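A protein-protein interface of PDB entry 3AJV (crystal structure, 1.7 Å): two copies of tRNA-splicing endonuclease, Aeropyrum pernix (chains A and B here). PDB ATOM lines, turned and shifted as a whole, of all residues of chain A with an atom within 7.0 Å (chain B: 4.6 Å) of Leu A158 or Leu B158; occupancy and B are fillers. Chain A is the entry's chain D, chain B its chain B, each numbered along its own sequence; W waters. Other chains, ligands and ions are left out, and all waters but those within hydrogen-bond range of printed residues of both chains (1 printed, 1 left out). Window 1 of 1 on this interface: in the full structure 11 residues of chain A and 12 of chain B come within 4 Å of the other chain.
Printed residues of chain B within 4 Å of Leu A158: Arg B157 and Leu B158.
Printed residues of chain A within 4 Å of Leu B158: Leu A158.
Of the printed residues of chain A, Arg B154 touches Gly A119 and Arg A154.
Printed residues of chain A within 4 Å of Arg B157: Phe A118 and Leu A158.
Printed residues of chain B within 4 Å of Gly A119: Arg B154.
Printed residues of chain B within 4 Å of Arg A157: Phe B118 and Gly B119.
The nearest printed residue of chain B that does not touch Leu A158 is Arg B154 (4.1 Å).
The nearest printed residue of chain A that does not touch Leu B158 is Arg A154 (4.01 Å).
The nearest printed residue of chain A that does not touch Arg B154 is Leu A158 (4.1 Å).
Water W1 bridges NH1 of Arg B154 and NH2 of Arg A154.
Phe A118 touches Arg B157.
Arg B154 touches Gly A119 (CG to O, 3.4 Å).
Arg A154 touches Gly B119 (CG to O, 3.3 Å).
Arg A157 touches Phe B118 (CG to C, 3.9 Å).
Arg A157 touches Gly B119.
CG of Arg B157 touches CD2 of Leu A158, 3.7 Å away.
Leu A158 touches Leu B158.
Gly A119 touches Arg B154, and with the chains exchanged Arg A154 touches Gly B119.
Arg B154 touches its own counterpart, Arg A154.
Arg A157 touches Gly B119, but with the chains exchanged Gly A119 does not touch Arg B157 (4.05 Å).
Leu A158 touches Arg B157, but with the chains exchanged Arg A157 does not touch Leu B158 (4.1 Å).
Of the 8 pairs that touch across the chains among the printed residues, 6 have their exchanged pair printed and touching as well.
Of the 11 printed residues of chain B, 5 touch a printed residue of chain A.
Hydrophobic or aromatic side chains of chain B that line the printed part of chain A: Leu B158.
Of the 19 printed residues of chain A, 5 touch a printed residue of chain B.
Hydrophobic or aromatic side chains of chain A that line the printed part of chain B: Leu A158.
Among the printed residues, no Asp or Glu carboxylate lies within 4 Å of a Lys or Arg side-chain nitrogen of the other chain.
NH1 of Arg B154 lies close to NH2 of Arg A154 (2.7 Å).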
ATOM      1  N   PHE A 118     -12.344 -27.203  25.791  1.00  0.00           N
ATOM      2  CA  PHE A 118     -12.982 -27.264  24.496  1.00  0.00           C
ATOM      3  C   PHE A 118     -13.397 -25.884  24.085  1.00  0.00           C
ATOM      4  O   PHE A 118     -14.059 -25.710  23.038  1.00  0.00           O
ATOM      5  CB  PHE A 118     -14.218 -28.151  24.571  1.00  0.00           C
ATOM      6  CG  PHE A 118     -13.910 -29.573  24.881  1.00  0.00           C
ATOM      7  CD1 PHE A 118     -13.462 -30.428  23.888  1.00  0.00           C
ATOM      8  CD2 PHE A 118     -14.034 -30.060  26.183  1.00  0.00           C
ATOM      9  CE1 PHE A 118     -13.146 -31.748  24.187  1.00  0.00           C
ATOM     10  CE2 PHE A 118     -13.719 -31.373  26.489  1.00  0.00           C
ATOM     11  CZ  PHE A 118     -13.277 -32.218  25.494  1.00  0.00           C
ATOM     12  N   GLY A 119     -13.051 -24.898  24.901  1.00  0.00           N
ATOM     13  CA  GLY A 119     -13.470 -23.504  24.658  1.00  0.00           C
ATOM     14  C   GLY A 119     -14.949 -23.162  24.894  1.00  0.00           C
ATOM     15  O   GLY A 119     -15.445 -22.121  24.367  1.00  0.00           O
ATOM     16  N   SER A 120     -15.667 -23.981  25.687  1.00  0.00           N
ATOM     17  CA  SER A 120     -17.116 -23.788  25.845  1.00  0.00           C
ATOM     18  C   SER A 120     -17.484 -23.679  27.319  1.00  0.00           C
ATOM     19  O   SER A 120     -16.595 -23.770  28.173  1.00  0.00           O
ATOM     20  CB  SER A 120     -17.919 -24.950  25.253  1.00  0.00           C
ATOM     21  OG  SER A 120     -17.578 -26.197  25.907  1.00  0.00           O
ATOM     22  N   ILE A 137     -20.449 -30.388  23.257  1.00  0.00           N
ATOM     23  CA  ILE A 137     -19.902 -29.126  23.642  1.00  0.00           C
ATOM     24  C   ILE A 137     -21.060 -28.123  23.708  1.00  0.00           C
ATOM     25  O   ILE A 137     -21.774 -27.885  22.743  1.00  0.00           O
ATOM     26  CB  ILE A 137     -18.811 -28.659  22.689  1.00  0.00           C
ATOM     27  CG1 ILE A 137     -17.703 -29.748  22.581  1.00  0.00           C
ATOM     28  CG2 ILE A 137     -18.307 -27.321  23.153  1.00  0.00           C
ATOM     29  CD1 ILE A 137     -17.341 -30.380  23.956  1.00  0.00           C
ATOM     30  N   HIS A 139     -22.723 -24.390  24.817  1.00  0.00           N
ATOM     31  CA  HIS A 139     -22.555 -22.955  24.945  1.00  0.00           C
ATOM     32  C   HIS A 139     -23.820 -22.414  25.613  1.00  0.00           C
ATOM     33  O   HIS A 139     -24.954 -22.723  25.148  1.00  0.00           O
ATOM     34  CB  HIS A 139     -22.379 -22.396  23.519  1.00  0.00           C
ATOM     35  CG  HIS A 139     -21.133 -22.889  22.837  1.00  0.00           C
ATOM     36  ND1 HIS A 139     -21.106 -23.999  22.021  1.00  0.00           N
ATOM     37  CD2 HIS A 139     -19.857 -22.451  22.916  1.00  0.00           C
ATOM     38  CE1 HIS A 139     -19.865 -24.212  21.609  1.00  0.00           C
ATOM     39  NE2 HIS A 139     -19.087 -23.298  22.147  1.00  0.00           N
ATOM     40  N   GLU A 151     -20.884 -15.729  15.232  1.00  0.00           N
ATOM     41  CA  GLU A 151     -20.634 -16.455  16.496  1.00  0.00           C
ATOM     42  C   GLU A 151     -21.055 -17.930  16.417  1.00  0.00           C
ATOM     43  O   GLU A 151     -20.483 -18.787  17.099  1.00  0.00           O
ATOM     44  CB  GLU A 151     -21.243 -15.718  17.696  1.00  0.00           C
ATOM     45  CG  GLU A 151     -20.627 -14.320  17.895  1.00  0.00           C
ATOM     46  CD  GLU A 151     -21.322 -13.487  18.956  1.00  0.00           C
ATOM     47  OE1 GLU A 151     -21.476 -13.992  20.103  1.00  0.00           O
ATOM     48  OE2 GLU A 151     -21.737 -12.339  18.649  1.00  0.00           O
ATOM     49  N   VAL A 153     -20.687 -19.757  13.683  1.00  0.00           N
ATOM     50  CA  VAL A 153     -19.539 -20.304  12.963  1.00  0.00           C
ATOM     51  C   VAL A 153     -18.347 -20.475  13.921  1.00  0.00           C
ATOM     52  O   VAL A 153     -17.628 -21.473  13.838  1.00  0.00           O
ATOM     53  CB  VAL A 153     -19.151 -19.492  11.719  1.00  0.00           C
ATOM     54  CG1 VAL A 153     -17.849 -20.059  11.073  1.00  0.00           C
ATOM     55  CG2 VAL A 153     -20.349 -19.430  10.704  1.00  0.00           C
ATOM     56  N   ARG A 154     -18.144 -19.513  14.820  1.00  0.00           N
ATOM     57  CA  ARG A 154     -17.081 -19.701  15.825  1.00  0.00           C
ATOM     58  C   ARG A 154     -17.316 -20.977  16.639  1.00  0.00           C
ATOM     59  O   ARG A 154     -16.353 -21.739  16.893  1.00  0.00           O
ATOM     60  CB  ARG A 154     -16.992 -18.510  16.777  1.00  0.00           C
ATOM     61  CG  ARG A 154     -15.824 -18.658  17.709  1.00  0.00           C
ATOM     62  CD  ARG A 154     -15.817 -17.464  18.654  1.00  0.00           C
ATOM     63  NE  ARG A 154     -16.952 -17.514  19.537  1.00  0.00           N
ATOM     64  CZ  ARG A 154     -17.398 -16.457  20.212  1.00  0.00           C
ATOM     65  NH1 ARG A 154     -16.776 -15.288  20.094  1.00  0.00           N
ATOM     66  NH2 ARG A 154     -18.444 -16.570  21.013  1.00  0.00           N
ATOM     67  N   ALA A 155     -18.561 -21.222  17.055  1.00  0.00           N
ATOM     68  CA  ALA A 155     -18.896 -22.458  17.764  1.00  0.00           C
ATOM     69  C   ALA A 155     -18.609 -23.699  16.911  1.00  0.00           C
ATOM     70  O   ALA A 155     -18.105 -24.724  17.427  1.00  0.00           O
ATOM     71  CB  ALA A 155     -20.363 -22.451  18.237  1.00  0.00           C
ATOM     72  N   GLY A 156     -18.919 -23.622  15.619  1.00  0.00           N
ATOM     73  CA  GLY A 156     -18.604 -24.684  14.681  1.00  0.00           C
ATOM     74  C   GLY A 156     -17.106 -24.937  14.645  1.00  0.00           C
ATOM     75  O   GLY A 156     -16.665 -26.080  14.599  1.00  0.00           O
ATOM     76  N   ARG A 157     -16.308 -23.877  14.689  1.00  0.00           N
ATOM     77  CA  ARG A 157     -14.843 -24.012  14.678  1.00  0.00           C
ATOM     78  C   ARG A 157     -14.316 -24.750  15.897  1.00  0.00           C
ATOM     79  O   ARG A 157     -13.458 -25.630  15.770  1.00  0.00           O
ATOM     80  CB  ARG A 157     -14.149 -22.647  14.574  1.00  0.00           C
ATOM     81  CG  ARG A 157     -13.300 -22.456  13.320  1.00  0.00           C
ATOM     82  CD  ARG A 157     -12.347 -23.630  13.044  1.00  0.00           C
ATOM     83  NE  ARG A 157     -10.935 -23.289  13.231  1.00  0.00           N
ATOM     84  CZ  ARG A 157      -9.938 -23.883  12.579  1.00  0.00           C
ATOM     85  NH1 ARG A 157     -10.198 -24.844  11.697  1.00  0.00           N
ATOM     86  NH2 ARG A 157      -8.680 -23.518  12.798  1.00  0.00           N
ATOM     87  N   LEU A 158     -14.802 -24.358  17.079  1.00  0.00           N
ATOM     88  CA  LEU A 158     -14.454 -25.019  18.322  1.00  0.00           C
ATOM     89  C   LEU A 158     -14.770 -26.511  18.274  1.00  0.00           C
ATOM     90  O   LEU A 158     -14.041 -27.325  18.852  1.00  0.00           O
ATOM     91  CB  LEU A 158     -15.177 -24.357  19.513  1.00  0.00           C
ATOM     92  CG  LEU A 158     -14.676 -22.940  19.803  1.00  0.00           C
ATOM     93  CD1 LEU A 158     -15.659 -22.144  20.650  1.00  0.00           C
ATOM     94  CD2 LEU A 158     -13.301 -23.024  20.466  1.00  0.00           C
ATOM     95  N   SER A 159     -15.828 -26.899  17.576  1.00  0.00           N
ATOM     96  CA  SER A 159     -16.217 -28.312  17.633  1.00  0.00           C
ATOM     97  C   SER A 159     -15.663 -29.127  16.461  1.00  0.00           C
ATOM     98  O   SER A 159     -15.860 -30.338  16.379  1.00  0.00           O
ATOM     99  CB  SER A 159     -17.733 -28.458  17.742  1.00  0.00           C
ATOM    100  OG  SER A 159     -18.181 -28.131  19.063  1.00  0.00           O
ATOM    101  N   HIS A 160     -14.952 -28.445  15.575  1.00  0.00           N
ATOM    102  CA  HIS A 160     -14.488 -29.007  14.302  1.00  0.00           C
ATOM    103  C   HIS A 160     -13.635 -30.279  14.428  1.00  0.00           C
ATOM    104  O   HIS A 160     -13.673 -31.162  13.551  1.00  0.00           O
ATOM    105  CB  HIS A 160     -13.747 -27.914  13.515  1.00  0.00           C
ATOM    106  CG  HIS A 160     -12.632 -28.427  12.659  1.00  0.00           C
ATOM    107  ND1 HIS A 160     -12.850 -29.154  11.508  1.00  0.00           N
ATOM    108  CD2 HIS A 160     -11.288 -28.306  12.779  1.00  0.00           C
ATOM    109  CE1 HIS A 160     -11.688 -29.471  10.963  1.00  0.00           C
ATOM    110  NE2 HIS A 160     -10.724 -28.963  11.713  1.00  0.00           N
ATOM    111  N   SER A 161     -12.870 -30.378  15.508  1.00  0.00           N
ATOM    112  CA  SER A 161     -11.976 -31.516  15.694  1.00  0.00           C
ATOM    113  C   SER A 161     -12.499 -32.562  16.689  1.00  0.00           C
ATOM    114  O   SER A 161     -11.923 -33.645  16.807  1.00  0.00           O
ATOM    115  CB  SER A 161     -10.594 -31.028  16.133  1.00  0.00           C
ATOM    116  OG  SER A 161      -9.578 -31.928  15.720  1.00  0.00           O
ATOM    117  N   VAL A 162     -13.581 -32.243  17.397  1.00  0.00           N
ATOM    118  CA  VAL A 162     -14.136 -33.137  18.423  1.00  0.00           C
ATOM    119  C   VAL A 162     -15.264 -33.975  17.834  1.00  0.00           C
ATOM    120  O   VAL A 162     -15.196 -35.215  17.743  1.00  0.00           O
ATOM    121  CB  VAL A 162     -14.772 -32.335  19.563  1.00  0.00           C
ATOM    122  CG1 VAL A 162     -13.855 -31.197  20.020  1.00  0.00           C
ATOM    123  CG2 VAL A 162     -16.125 -31.793  19.114  1.00  0.00           C
ATOM    124  N   ARG A 163     -16.329 -33.253  17.521  1.00  0.00           N
ATOM    125  CA  ARG A 163     -17.385 -33.661  16.635  1.00  0.00           C
ATOM    126  C   ARG A 163     -17.875 -32.335  16.060  1.00  0.00           C
ATOM    127  O   ARG A 163     -17.889 -31.332  16.760  1.00  0.00           O
ATOM    128  CB  ARG A 163     -18.485 -34.378  17.409  1.00  0.00           C
ATOM    129  CG  ARG A 163     -18.588 -35.859  17.081  1.00  0.00           C
ATOM    130  CD  ARG A 163     -17.349 -36.687  17.449  1.00  0.00           C
ATOM    131  NE  ARG A 163     -17.487 -38.045  16.929  1.00  0.00           N
ATOM    132  CZ  ARG A 163     -16.887 -39.124  17.431  1.00  0.00           C
ATOM    133  NH1 ARG A 163     -17.087 -40.315  16.868  1.00  0.00           N
ATOM    134  NH2 ARG A 163     -16.092 -39.020  18.488  1.00  0.00           N
ATOM    135  N   LYS A 165     -20.411 -31.238  15.747  1.00  0.00           N
ATOM    136  CA  LYS A 165     -21.723 -30.982  16.323  1.00  0.00           C
ATOM    137  C   LYS A 165     -21.553 -30.208  17.630  1.00  0.00           C
ATOM    138  O   LYS A 165     -20.479 -30.253  18.257  1.00  0.00           O
ATOM    139  CB  LYS A 165     -22.437 -32.318  16.538  1.00  0.00           C
ATOM    140  CG  LYS A 165     -23.889 -32.210  16.952  1.00  0.00           C
ATOM    141  CD  LYS A 165     -24.757 -33.296  16.317  1.00  0.00           C
ATOM    142  CE  LYS A 165     -26.216 -33.027  16.661  1.00  0.00           C
ATOM    143  NZ  LYS A 165     -26.182 -32.073  17.847  1.00  0.00           N
ATOM    144  N   PHE A 166     -22.566 -29.458  18.025  1.00  0.00           N
ATOM    145  CA  PHE A 166     -22.413 -28.634  19.209  1.00  0.00           C
ATOM    146  C   PHE A 166     -23.796 -28.124  19.593  1.00  0.00           C
ATOM    147  O   PHE A 166     -24.744 -28.326  18.863  1.00  0.00           O
ATOM    148  CB  PHE A 166     -21.408 -27.496  19.007  1.00  0.00           C
ATOM    149  CG  PHE A 166     -21.732 -26.582  17.864  1.00  0.00           C
ATOM    150  CD1 PHE A 166     -22.428 -25.408  18.071  1.00  0.00           C
ATOM    151  CD2 PHE A 166     -21.304 -26.909  16.573  1.00  0.00           C
ATOM    152  CE1 PHE A 166     -22.703 -24.542  16.994  1.00  0.00           C
ATOM    153  CE2 PHE A 166     -21.584 -26.070  15.518  1.00  0.00           C
ATOM    154  CZ  PHE A 166     -22.255 -24.884  15.739  1.00  0.00           C
ATOM    155  N   PHE B 118     -11.173 -19.307  11.086  1.00  0.00           N
ATOM    156  CA  PHE B 118     -10.377 -19.501  12.288  1.00  0.00           C
ATOM    157  C   PHE B 118     -11.189 -19.166  13.531  1.00  0.00           C
ATOM    158  O   PHE B 118     -10.659 -19.142  14.654  1.00  0.00           O
ATOM    159  CB  PHE B 118      -9.109 -18.638  12.237  1.00  0.00           C
ATOM    160  CG  PHE B 118      -8.188 -18.992  11.127  1.00  0.00           C
ATOM    161  CD1 PHE B 118      -7.271 -20.015  11.272  1.00  0.00           C
ATOM    162  CD2 PHE B 118      -8.241 -18.310   9.921  1.00  0.00           C
ATOM    163  CE1 PHE B 118      -6.436 -20.371  10.231  1.00  0.00           C
ATOM    164  CE2 PHE B 118      -7.397 -18.648   8.864  1.00  0.00           C
ATOM    165  CZ  PHE B 118      -6.491 -19.675   9.017  1.00  0.00           C
ATOM    166  N   GLY B 119     -12.457 -18.863  13.319  1.00  0.00           N
ATOM    167  CA  GLY B 119     -13.379 -18.453  14.380  1.00  0.00           C
ATOM    168  C   GLY B 119     -13.122 -17.077  14.989  1.00  0.00           C
ATOM    169  O   GLY B 119     -13.480 -16.853  16.158  1.00  0.00           O
ATOM    170  N   HIS B 139      -8.871 -10.963  17.473  1.00  0.00           N
ATOM    171  CA  HIS B 139     -10.141 -10.729  18.060  1.00  0.00           C
ATOM    172  C   HIS B 139     -10.288  -9.228  18.395  1.00  0.00           C
ATOM    173  O   HIS B 139      -9.403  -8.636  19.047  1.00  0.00           O
ATOM    174  CB  HIS B 139     -10.179 -11.527  19.363  1.00  0.00           C
ATOM    175  CG  HIS B 139      -9.915 -12.996  19.177  1.00  0.00           C
ATOM    176  ND1 HIS B 139      -8.646 -13.537  19.088  1.00  0.00           N
ATOM    177  CD2 HIS B 139     -10.773 -14.031  19.046  1.00  0.00           C
ATOM    178  CE1 HIS B 139      -8.740 -14.844  18.880  1.00  0.00           C
ATOM    179  NE2 HIS B 139     -10.015 -15.175  18.896  1.00  0.00           N
ATOM    180  N   ARG B 154     -10.795 -19.419  25.700  1.00  0.00           N
ATOM    181  CA  ARG B 154     -11.505 -19.814  24.472  1.00  0.00           C
ATOM    182  C   ARG B 154     -10.672 -19.383  23.256  1.00  0.00           C
ATOM    183  O   ARG B 154     -10.458 -20.198  22.318  1.00  0.00           O
ATOM    184  CB  ARG B 154     -12.907 -19.194  24.379  1.00  0.00           C
ATOM    185  CG  ARG B 154     -13.624 -19.603  23.087  1.00  0.00           C
ATOM    186  CD  ARG B 154     -14.959 -18.871  22.950  1.00  0.00           C
ATOM    187  NE  ARG B 154     -14.809 -17.428  22.880  1.00  0.00           N
ATOM    188  CZ  ARG B 154     -15.809 -16.574  23.065  1.00  0.00           C
ATOM    189  NH1 ARG B 154     -17.037 -17.033  23.301  1.00  0.00           N
ATOM    190  NH2 ARG B 154     -15.591 -15.269  22.978  1.00  0.00           N
ATOM    191  N   ALA B 155     -10.135 -18.159  23.302  1.00  0.00           N
ATOM    192  CA  ALA B 155      -9.263 -17.662  22.246  1.00  0.00           C
ATOM    193  C   ALA B 155      -8.064 -18.568  22.057  1.00  0.00           C
ATOM    194  O   ALA B 155      -7.650 -18.880  20.936  1.00  0.00           O
ATOM    195  CB  ALA B 155      -8.826 -16.223  22.553  1.00  0.00           C
ATOM    196  N   GLY B 156      -7.480 -18.986  23.167  1.00  0.00           N
ATOM    197  CA  GLY B 156      -6.388 -19.903  23.102  1.00  0.00           C
ATOM    198  C   GLY B 156      -6.751 -21.213  22.438  1.00  0.00           C
ATOM    199  O   GLY B 156      -5.928 -21.771  21.723  1.00  0.00           O
ATOM    200  N   ARG B 157      -7.973 -21.718  22.633  1.00  0.00           N
ATOM    201  CA  ARG B 157      -8.390 -22.993  22.047  1.00  0.00           C
ATOM    202  C   ARG B 157      -8.510 -22.857  20.546  1.00  0.00           C
ATOM    203  O   ARG B 157      -8.152 -23.770  19.790  1.00  0.00           O
ATOM    204  CB  ARG B 157      -9.748 -23.439  22.613  1.00  0.00           C
ATOM    205  CG  ARG B 157     -10.340 -24.662  21.905  1.00  0.00           C
ATOM    206  CD  ARG B 157      -9.627 -25.949  22.310  1.00  0.00           C
ATOM    207  NE  ARG B 157     -10.308 -27.141  21.814  1.00  0.00           N
ATOM    208  CZ  ARG B 157      -9.756 -28.349  21.757  1.00  0.00           C
ATOM    209  NH1 ARG B 157      -8.504 -28.538  22.164  1.00  0.00           N
ATOM    210  NH2 ARG B 157     -10.455 -29.378  21.292  1.00  0.00           N
ATOM    211  N   LEU B 158      -9.026 -21.702  20.123  1.00  0.00           N
ATOM    212  CA  LEU B 158      -9.173 -21.383  18.714  1.00  0.00           C
ATOM    213  C   LEU B 158      -7.827 -21.313  18.020  1.00  0.00           C
ATOM    214  O   LEU B 158      -7.730 -21.613  16.835  1.00  0.00           O
ATOM    215  CB  LEU B 158      -9.914 -20.056  18.503  1.00  0.00           C
ATOM    216  CG  LEU B 158     -11.412 -20.136  18.792  1.00  0.00           C
ATOM    217  CD1 LEU B 158     -12.029 -18.772  18.987  1.00  0.00           C
ATOM    218  CD2 LEU B 158     -12.099 -20.885  17.677  1.00  0.00           C
ATOM    219  N   SER B 159      -6.780 -20.914  18.731  1.00  0.00           N
ATOM    220  CA  SER B 159      -5.505 -20.757  18.030  1.00  0.00           C
ATOM    221  C   SER B 159      -4.598 -21.961  18.214  1.00  0.00           C
ATOM    222  O   SER B 159      -3.502 -22.010  17.664  1.00  0.00           O
ATOM    223  CB  SER B 159      -4.782 -19.476  18.439  1.00  0.00           C
ATOM    224  OG  SER B 159      -5.322 -18.368  17.734  1.00  0.00           O
ATOM    225  N   HIS B 160      -5.071 -22.930  18.983  1.00  0.00           N
ATOM    226  CA  HIS B 160      -4.245 -24.059  19.375  1.00  0.00           C
ATOM    227  C   HIS B 160      -3.691 -24.904  18.225  1.00  0.00           C
ATOM    228  O   HIS B 160      -2.614 -25.510  18.357  1.00  0.00           O
ATOM    229  CB  HIS B 160      -4.976 -24.922  20.405  1.00  0.00           C
ATOM    230  CG  HIS B 160      -4.315 -24.928  21.749  1.00  0.00           C
ATOM    231  ND1 HIS B 160      -4.532 -23.947  22.694  1.00  0.00           N
ATOM    232  CD2 HIS B 160      -3.420 -25.785  22.293  1.00  0.00           C
ATOM    233  CE1 HIS B 160      -3.806 -24.206  23.767  1.00  0.00           C
ATOM    234  NE2 HIS B 160      -3.125 -25.318  23.551  1.00  0.00           N
ATOM    235  N   VAL B 162      -2.980 -23.565  15.259  1.00  0.00           N
ATOM    236  CA  VAL B 162      -2.536 -22.584  14.266  1.00  0.00           C
ATOM    237  C   VAL B 162      -1.124 -22.028  14.507  1.00  0.00           C
ATOM    238  O   VAL B 162      -0.231 -22.162  13.681  1.00  0.00           O
ATOM    239  CB  VAL B 162      -3.527 -21.375  14.216  1.00  0.00           C
ATOM    240  CG1 VAL B 162      -3.089 -20.358  13.217  1.00  0.00           C
ATOM    241  CG2 VAL B 162      -4.950 -21.826  13.845  1.00  0.00           C
HETATM  242  O   HOH W   1     -19.696 -15.698  23.825  1.00  0.00           O
